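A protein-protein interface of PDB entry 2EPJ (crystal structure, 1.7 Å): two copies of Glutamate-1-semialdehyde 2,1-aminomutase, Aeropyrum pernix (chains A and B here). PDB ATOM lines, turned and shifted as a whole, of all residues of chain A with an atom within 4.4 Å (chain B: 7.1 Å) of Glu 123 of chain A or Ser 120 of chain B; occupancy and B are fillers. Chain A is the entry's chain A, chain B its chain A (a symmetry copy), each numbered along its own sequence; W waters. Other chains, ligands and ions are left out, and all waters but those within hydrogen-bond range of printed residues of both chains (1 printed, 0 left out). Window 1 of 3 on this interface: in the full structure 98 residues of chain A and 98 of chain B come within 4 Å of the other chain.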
ATOM      1  N   VAL A 118      35.303  -2.202   9.970  1.00  0.00           N
ATOM      2  CA  VAL A 118      34.230  -1.503   9.280  1.00  0.00           C
ATOM      3  C   VAL A 118      34.842  -0.502   8.293  1.00  0.00           C
ATOM      4  O   VAL A 118      36.045  -0.557   8.023  1.00  0.00           O
ATOM      5  CB  VAL A 118      33.252  -0.824  10.276  1.00  0.00           C
ATOM      6  CG1 VAL A 118      32.526  -1.902  11.076  1.00  0.00           C
ATOM      7  CG2 VAL A 118      33.988   0.118  11.203  1.00  0.00           C
ATOM      8  N   ASN A 119      34.048   0.431   7.778  1.00  0.00           N
ATOM      9  CA  ASN A 119      34.558   1.326   6.741  1.00  0.00           C
ATOM     10  C   ASN A 119      34.801   2.802   7.015  1.00  0.00           C
ATOM     11  O   ASN A 119      35.191   3.552   6.112  1.00  0.00           O
ATOM     12  CB  ASN A 119      33.657   1.141   5.532  1.00  0.00           C
ATOM     13  CG  ASN A 119      33.451  -0.324   5.221  1.00  0.00           C
ATOM     14  OD1 ASN A 119      34.322  -0.973   4.644  1.00  0.00           O
ATOM     15  ND2 ASN A 119      32.313  -0.866   5.647  1.00  0.00           N
ATOM     16  N   SER A 120      34.586   3.218   8.255  1.00  0.00           N
ATOM     17  CA  SER A 120      34.820   4.602   8.636  1.00  0.00           C
ATOM     18  C   SER A 120      34.843   4.681  10.154  1.00  0.00           C
ATOM     19  O   SER A 120      34.404   3.753  10.834  1.00  0.00           O
ATOM     20  CB  SER A 120      33.713   5.514   8.098  1.00  0.00           C
ATOM     21  OG  SER A 120      32.471   5.225   8.718  1.00  0.00           O
ATOM     22  N   GLY A 121      35.369   5.784  10.678  1.00  0.00           N
ATOM     23  CA  GLY A 121      35.403   5.967  12.117  1.00  0.00           C
ATOM     24  C   GLY A 121      33.975   6.109  12.606  1.00  0.00           C
ATOM     25  O   GLY A 121      33.640   5.695  13.718  1.00  0.00           O
ATOM     26  N   THR A 122      33.131   6.702  11.764  1.00  0.00           N
ATOM     27  CA  THR A 122      31.719   6.892  12.075  1.00  0.00           C
ATOM     28  C   THR A 122      31.052   5.530  12.263  1.00  0.00           C
ATOM     29  O   THR A 122      30.351   5.308  13.246  1.00  0.00           O
ATOM     30  CB  THR A 122      30.998   7.668  10.942  1.00  0.00           C
ATOM     31  OG1 THR A 122      31.444   9.030  10.936  1.00  0.00           O
ATOM     32  CG2 THR A 122      29.484   7.640  11.138  1.00  0.00           C
ATOM     33  N   GLU A 123      31.267   4.616  11.323  1.00  0.00           N
ATOM     34  CA  GLU A 123      30.674   3.288  11.455  1.00  0.00           C
ATOM     35  C   GLU A 123      31.221   2.602  12.702  1.00  0.00           C
ATOM     36  O   GLU A 123      30.498   1.891  13.402  1.00  0.00           O
ATOM     37  CB  GLU A 123      30.985   2.413  10.236  1.00  0.00           C
ATOM     38  CG  GLU A 123      30.272   2.805   8.946  1.00  0.00           C
ATOM     39  CD  GLU A 123      30.266   1.671   7.934  1.00  0.00           C
ATOM     40  OE1 GLU A 123      31.324   1.029   7.753  1.00  0.00           O
ATOM     41  OE2 GLU A 123      29.207   1.419   7.319  1.00  0.00           O
ATOM     42  N   ALA A 124      32.503   2.822  12.978  1.00  0.00           N
ATOM     43  CA  ALA A 124      33.150   2.205  14.130  1.00  0.00           C
ATOM     44  C   ALA A 124      32.557   2.634  15.471  1.00  0.00           C
ATOM     45  O   ALA A 124      32.216   1.784  16.299  1.00  0.00           O
ATOM     46  CB  ALA A 124      34.652   2.494  14.100  1.00  0.00           C
ATOM     47  N   THR A 125      32.424   3.939  15.697  1.00  0.00           N
ATOM     48  CA  THR A 125      31.876   4.396  16.974  1.00  0.00           C
ATOM     49  C   THR A 125      30.403   4.020  17.094  1.00  0.00           C
ATOM     50  O   THR A 125      29.923   3.693  18.176  1.00  0.00           O
ATOM     51  CB  THR A 125      32.049   5.925  17.167  1.00  0.00           C
ATOM     52  OG1 THR A 125      31.277   6.639  16.194  1.00  0.00           O
ATOM     53  CG2 THR A 125      33.517   6.307  17.022  1.00  0.00           C
ATOM     54  N   MET A 126      29.695   4.055  15.971  1.00  0.00           N
ATOM     55  CA  MET A 126      28.285   3.700  15.938  1.00  0.00           C
ATOM     56  C   MET A 126      28.120   2.229  16.352  1.00  0.00           C
ATOM     57  O   MET A 126      27.221   1.877  17.123  1.00  0.00           O
ATOM     58  CB  MET A 126      27.761   3.939  14.520  1.00  0.00           C
ATOM     59  CG  MET A 126      26.334   3.554  14.263  1.00  0.00           C
ATOM     60  SD  MET A 126      25.901   4.083  12.586  1.00  0.00           S
ATOM     61  CE  MET A 126      26.627   2.780  11.594  1.00  0.00           C
ATOM     62  N   THR A 127      29.005   1.377  15.848  1.00  0.00           N
ATOM     63  CA  THR A 127      28.964  -0.043  16.170  1.00  0.00           C
ATOM     64  C   THR A 127      29.337  -0.265  17.638  1.00  0.00           C
ATOM     65  O   THR A 127      28.738  -1.096  18.323  1.00  0.00           O
ATOM     66  CB  THR A 127      29.932  -0.835  15.259  1.00  0.00           C
ATOM     67  OG1 THR A 127      29.592  -0.600  13.886  1.00  0.00           O
ATOM     68  CG2 THR A 127      29.839  -2.332  15.544  1.00  0.00           C
ATOM     69  N   PHE B 117      29.268  12.067  -1.497  1.00  0.00           N
ATOM     70  CA  PHE B 117      29.893  10.748  -1.447  1.00  0.00           C
ATOM     71  C   PHE B 117      30.251  10.347  -0.024  1.00  0.00           C
ATOM     72  O   PHE B 117      30.828  11.138   0.723  1.00  0.00           O
ATOM     73  CB  PHE B 117      31.172  10.719  -2.295  1.00  0.00           C
ATOM     74  CG  PHE B 117      30.928  10.805  -3.776  1.00  0.00           C
ATOM     75  CD1 PHE B 117      30.212   9.813  -4.436  1.00  0.00           C
ATOM     76  CD2 PHE B 117      31.437  11.869  -4.515  1.00  0.00           C
ATOM     77  CE1 PHE B 117      30.006   9.874  -5.815  1.00  0.00           C
ATOM     78  CE2 PHE B 117      31.238  11.943  -5.895  1.00  0.00           C
ATOM     79  CZ  PHE B 117      30.521  10.941  -6.548  1.00  0.00           C
ATOM     80  N   VAL B 118      29.902   9.119   0.346  1.00  0.00           N
ATOM     81  CA  VAL B 118      30.229   8.597   1.665  1.00  0.00           C
ATOM     82  C   VAL B 118      30.981   7.271   1.503  1.00  0.00           C
ATOM     83  O   VAL B 118      31.411   6.936   0.396  1.00  0.00           O
ATOM     84  CB  VAL B 118      28.967   8.454   2.556  1.00  0.00           C
ATOM     85  CG1 VAL B 118      28.400   9.841   2.845  1.00  0.00           C
ATOM     86  CG2 VAL B 118      27.925   7.585   1.886  1.00  0.00           C
ATOM     87  N   ASN B 119      31.114   6.495   2.574  1.00  0.00           N
ATOM     88  CA  ASN B 119      31.928   5.285   2.496  1.00  0.00           C
ATOM     89  C   ASN B 119      31.300   3.901   2.547  1.00  0.00           C
ATOM     90  O   ASN B 119      32.010   2.887   2.523  1.00  0.00           O
ATOM     91  CB  ASN B 119      33.012   5.425   3.551  1.00  0.00           C
ATOM     92  CG  ASN B 119      33.678   6.781   3.475  1.00  0.00           C
ATOM     93  OD1 ASN B 119      34.519   7.021   2.610  1.00  0.00           O
ATOM     94  ND2 ASN B 119      33.268   7.693   4.352  1.00  0.00           N
ATOM     95  N   SER B 120      29.977   3.852   2.602  1.00  0.00           N
ATOM     96  CA  SER B 120      29.269   2.581   2.620  1.00  0.00           C
ATOM     97  C   SER B 120      27.803   2.847   2.317  1.00  0.00           C
ATOM     98  O   SER B 120      27.348   3.988   2.390  1.00  0.00           O
ATOM     99  CB  SER B 120      29.390   1.905   3.988  1.00  0.00           C
ATOM    100  OG  SER B 120      28.712   2.653   4.986  1.00  0.00           O
ATOM    101  N   GLY B 121      27.075   1.792   1.964  1.00  0.00           N
ATOM    102  CA  GLY B 121      25.658   1.940   1.689  1.00  0.00           C
ATOM    103  C   GLY B 121      24.965   2.305   2.987  1.00  0.00           C
ATOM    104  O   GLY B 121      23.972   3.036   2.993  1.00  0.00           O
ATOM    105  N   THR B 122      25.495   1.786   4.093  1.00  0.00           N
ATOM    106  CA  THR B 122      24.961   2.061   5.422  1.00  0.00           C
ATOM    107  C   THR B 122      25.062   3.559   5.711  1.00  0.00           C
ATOM    108  O   THR B 122      24.092   4.180   6.134  1.00  0.00           O
ATOM    109  CB  THR B 122      25.736   1.273   6.509  1.00  0.00           C
ATOM    110  OG1 THR B 122      25.432  -0.124   6.395  1.00  0.00           O
ATOM    111  CG2 THR B 122      25.356   1.753   7.908  1.00  0.00           C
ATOM    112  N   GLU B 123      26.234   4.142   5.482  1.00  0.00           N
ATOM    113  CA  GLU B 123      26.389   5.574   5.719  1.00  0.00           C
ATOM    114  C   GLU B 123      25.457   6.352   4.796  1.00  0.00           C
ATOM    115  O   GLU B 123      24.887   7.372   5.185  1.00  0.00           O
ATOM    116  CB  GLU B 123      27.829   6.031   5.462  1.00  0.00           C
ATOM    117  CG  GLU B 123      28.859   5.563   6.486  1.00  0.00           C
ATOM    118  CD  GLU B 123      30.130   6.395   6.433  1.00  0.00           C
ATOM    119  OE1 GLU B 123      30.616   6.667   5.313  1.00  0.00           O
ATOM    120  OE2 GLU B 123      30.645   6.776   7.506  1.00  0.00           O
ATOM    121  N   ALA B 124      25.305   5.863   3.569  1.00  0.00           N
ATOM    122  CA  ALA B 124      24.458   6.527   2.585  1.00  0.00           C
ATOM    123  C   ALA B 124      22.985   6.592   2.984  1.00  0.00           C
ATOM    124  O   ALA B 124      22.380   7.667   2.952  1.00  0.00           O
ATOM    125  CB  ALA B 124      24.607   5.843   1.224  1.00  0.00           C
ATOM    126  N   THR B 125      22.399   5.458   3.364  1.00  0.00           N
ATOM    127  CA  THR B 125      20.986   5.471   3.739  1.00  0.00           C
ATOM    128  C   THR B 125      20.778   6.248   5.034  1.00  0.00           C
ATOM    129  O   THR B 125      19.771   6.930   5.205  1.00  0.00           O
ATOM    130  CB  THR B 125      20.411   4.038   3.884  1.00  0.00           C
ATOM    131  OG1 THR B 125      21.043   3.357   4.975  1.00  0.00           O
ATOM    132  CG2 THR B 125      20.639   3.250   2.600  1.00  0.00           C
ATOM    133  N   MET B 126      21.746   6.151   5.938  1.00  0.00           N
ATOM    134  CA  MET B 126      21.687   6.857   7.209  1.00  0.00           C
ATOM    135  C   MET B 126      21.668   8.371   6.950  1.00  0.00           C
ATOM    136  O   MET B 126      20.909   9.119   7.574  1.00  0.00           O
ATOM    137  CB  MET B 126      22.905   6.452   8.042  1.00  0.00           C
ATOM    138  CG  MET B 126      23.066   7.140   9.365  1.00  0.00           C
ATOM    139  SD  MET B 126      24.464   6.380  10.229  1.00  0.00           S
ATOM    140  CE  MET B 126      25.859   7.176   9.435  1.00  0.00           C
ATOM    141  N   SER B 151      23.602  -1.276   8.196  1.00  0.00           N
ATOM    142  CA  SER B 151      23.804  -1.535   9.607  1.00  0.00           C
ATOM    143  C   SER B 151      23.707  -0.320  10.534  1.00  0.00           C
ATOM    144  O   SER B 151      24.666   0.017  11.225  1.00  0.00           O
ATOM    145  CB  SER B 151      25.164  -2.229   9.778  1.00  0.00           C
ATOM    146  OG  SER B 151      25.371  -2.679  11.102  1.00  0.00           O
ATOM    147  N   VAL B 245      21.239   1.202  -3.818  1.00  0.00           N
ATOM    148  CA  VAL B 245      22.596   0.755  -3.549  1.00  0.00           C
ATOM    149  C   VAL B 245      22.914  -0.448  -4.438  1.00  0.00           C
ATOM    150  O   VAL B 245      24.044  -0.593  -4.908  1.00  0.00           O
ATOM    151  CB  VAL B 245      22.773   0.411  -2.050  1.00  0.00           C
ATOM    152  CG1 VAL B 245      24.056  -0.380  -1.825  1.00  0.00           C
ATOM    153  CG2 VAL B 245      22.821   1.703  -1.246  1.00  0.00           C
ATOM    154  N   VAL B 268      19.684   6.835  -3.159  1.00  0.00           N
ATOM    155  CA  VAL B 268      20.839   6.326  -2.430  1.00  0.00           C
ATOM    156  C   VAL B 268      21.585   5.382  -3.366  1.00  0.00           C
ATOM    157  O   VAL B 268      20.990   4.476  -3.951  1.00  0.00           O
ATOM    158  CB  VAL B 268      20.417   5.560  -1.163  1.00  0.00           C
ATOM    159  CG1 VAL B 268      21.647   5.273  -0.299  1.00  0.00           C
ATOM    160  CG2 VAL B 268      19.402   6.376  -0.377  1.00  0.00           C
ATOM    161  N   LEU B 269      22.885   5.608  -3.518  1.00  0.00           N
ATOM    162  CA  LEU B 269      23.703   4.783  -4.396  1.00  0.00           C
ATOM    163  C   LEU B 269      24.854   4.145  -3.631  1.00  0.00           C
ATOM    164  O   LEU B 269      25.189   4.564  -2.522  1.00  0.00           O
ATOM    165  CB  LEU B 269      24.260   5.632  -5.543  1.00  0.00           C
ATOM    166  CG  LEU B 269      23.244   6.283  -6.488  1.00  0.00           C
ATOM    167  CD1 LEU B 269      23.961   7.282  -7.386  1.00  0.00           C
ATOM    168  CD2 LEU B 269      22.549   5.215  -7.322  1.00  0.00           C
ATOM    169  N   GLY B 270      25.458   3.130  -4.236  1.00  0.00           N
ATOM    170  CA  GLY B 270      26.570   2.454  -3.605  1.00  0.00           C
ATOM    171  C   GLY B 270      27.111   1.366  -4.505  1.00  0.00           C
ATOM    172  O   GLY B 270      26.964   1.427  -5.726  1.00  0.00           O
ATOM    173  N   LYS B 271      27.744   0.377  -3.886  1.00  0.00           N
ATOM    174  CA  LYS B 271      28.317  -0.767  -4.581  1.00  0.00           C
ATOM    175  C   LYS B 271      28.968  -0.472  -5.936  1.00  0.00           C
ATOM    176  O   LYS B 271      30.119  -0.052  -5.979  1.00  0.00           O
ATOM    177  CB  LYS B 271      27.256  -1.866  -4.698  1.00  0.00           C
ATOM    178  CG  LYS B 271      26.844  -2.399  -3.323  1.00  0.00           C
ATOM    179  CD  LYS B 271      25.875  -3.572  -3.397  1.00  0.00           C
ATOM    180  CE  LYS B 271      25.750  -4.224  -2.026  1.00  0.00           C
ATOM    181  NZ  LYS B 271      24.775  -5.343  -1.990  1.00  0.00           N
ATOM    182  N   PRO B 278      35.291   0.909  -1.167  1.00  0.00           N
ATOM    183  CA  PRO B 278      34.304   1.439  -0.214  1.00  0.00           C
ATOM    184  C   PRO B 278      33.601   2.689  -0.716  1.00  0.00           C
ATOM    185  O   PRO B 278      34.246   3.681  -1.051  1.00  0.00           O
ATOM    186  CB  PRO B 278      35.134   1.697   1.040  1.00  0.00           C
ATOM    187  CG  PRO B 278      36.209   0.648   0.952  1.00  0.00           C
ATOM    188  CD  PRO B 278      36.601   0.737  -0.511  1.00  0.00           C
ATOM    189  N   VAL B 279      32.274   2.644  -0.757  1.00  0.00           N
ATOM    190  CA  VAL B 279      31.524   3.778  -1.270  1.00  0.00           C
ATOM    191  C   VAL B 279      30.049   3.775  -0.885  1.00  0.00           C
ATOM    192  O   VAL B 279      29.483   2.752  -0.475  1.00  0.00           O
ATOM    193  CB  VAL B 279      31.612   3.807  -2.819  1.00  0.00           C
ATOM    194  CG1 VAL B 279      30.755   2.684  -3.404  1.00  0.00           C
ATOM    195  CG2 VAL B 279      31.179   5.166  -3.364  1.00  0.00           C
ATOM    196  N   GLY B 280      29.450   4.949  -1.046  1.00  0.00           N
ATOM    197  CA  GLY B 280      28.044   5.172  -0.788  1.00  0.00           C
ATOM    198  C   GLY B 280      27.797   6.579  -1.300  1.00  0.00           C
ATOM    199  O   GLY B 280      28.743   7.356  -1.431  1.00  0.00           O
ATOM    200  N   ALA B 281      26.554   6.919  -1.615  1.00  0.00           N
ATOM    201  CA  ALA B 281      26.259   8.270  -2.076  1.00  0.00           C
ATOM    202  C   ALA B 281      24.788   8.597  -1.922  1.00  0.00           C
ATOM    203  O   ALA B 281      23.932   7.709  -1.931  1.00  0.00           O
ATOM    204  CB  ALA B 281      26.679   8.448  -3.540  1.00  0.00           C
HETATM  205  O   HOH W   1      27.281  -1.007  12.358  1.00  0.00           O
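Asn 119 of chain B touches its own counterpart, Asn 119 of chain A.
Ser 120 of chain A touches Glu 123 of chain B, and with the chains exchanged Glu 123 of chain A touches Ser 120 of chain B.
Glu 123 of chain A touches its own counterpart, Glu 123 of chain B.
Met 126 of chain B touches its own counterpart, Met 126 of chain A.
Positions printed for both chains: 118, 119, 120, 121, 122, 123, 124, 125 and 126.
Among the printed residues, merely in contact across the chains: Met 126 of chain A with Ser 151 of chain B (3.4 Å), Glu 123 of chain A with Thr 122 of chain B (3.6 Å), Thr 122 of chain A with Glu 123 of chain B (3.6 Å), Asn 119 of chain A with Asn 119 of chain B (3.8 Å) and Glu 123 of chain A with Glu 123 of chain B (3.96 Å).
Glu 123 of chain A touches three residues of chain B.
Ser 120 of chain B touches just one residue of chain A: Glu 123 (2.7 Å).
Of the printed residues of chain A, Met 126 of chain B touches Met 126 (3.6 Å).
Of the printed residues of chain A, Thr 122 of chain B touches Glu 123.
Printed residues of chain B within 4 Å of Met 126 of chain A: Met 126 (3.6 Å) and Ser 151 (3.4 Å).
Printed residues of chain B within 4 Å of Asn 119 of chain A: Asn 119 (3.8 Å).
Printed residues of chain A within 4 Å of Ser 151 of chain B: Met 126.
Water W1 bridges OG1 of Thr 127 of chain A and OG of Ser 151 of chain B.
The backbone carbonyl oxygen (O) of Thr 122 of chain B sits at hydrogen-bond distance from the side-chain hydroxyl (OG1) of Thr 125 of chain B, 3.4 Å away.
The backbone NH (N) of Ser 120 of chain B lies close to the backbone carbonyl oxygen (O) of Val 279 of chain B (3.3 Å).
The backbone NH (N) of Asn 119 of chain A lies within hydrogen-bond range of the side-chain carboxylate (OE1) of Glu 123 of chain A.
The backbone carbonyl oxygen (O) of Asn 119 of chain B is in hydrogen-bond range of the backbone NH (N) of Val 279 of chain B (3.3 Å).
The backbone NH of Thr 122 of chain A lies close to the side-chain hydroxyl of Ser 120 of chain A (3.4 Å).
The side-chain hydroxyl (OG) of Ser 120 of chain B lies close to the backbone NH (N) of Thr 122 of chain B, at 3.4 Å.
Among the printed residues, no Asp or Glu carboxylate lies within 4 Å of a Lys or Arg side-chain nitrogen of the other chain.
OG of Ser 120 of chain A sits at hydrogen-bond distance from OE2 of Glu 123 of chain B.
SD of Met 126 of chain A sits close to SD of Met 126 of chain B (3.6 Å).
The side-chain carboxylate (OE2) of Glu 123 of chain A is in hydrogen-bond range of the side-chain hydroxyl (OG) of Ser 120 of chain B, 2.7 Å away.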
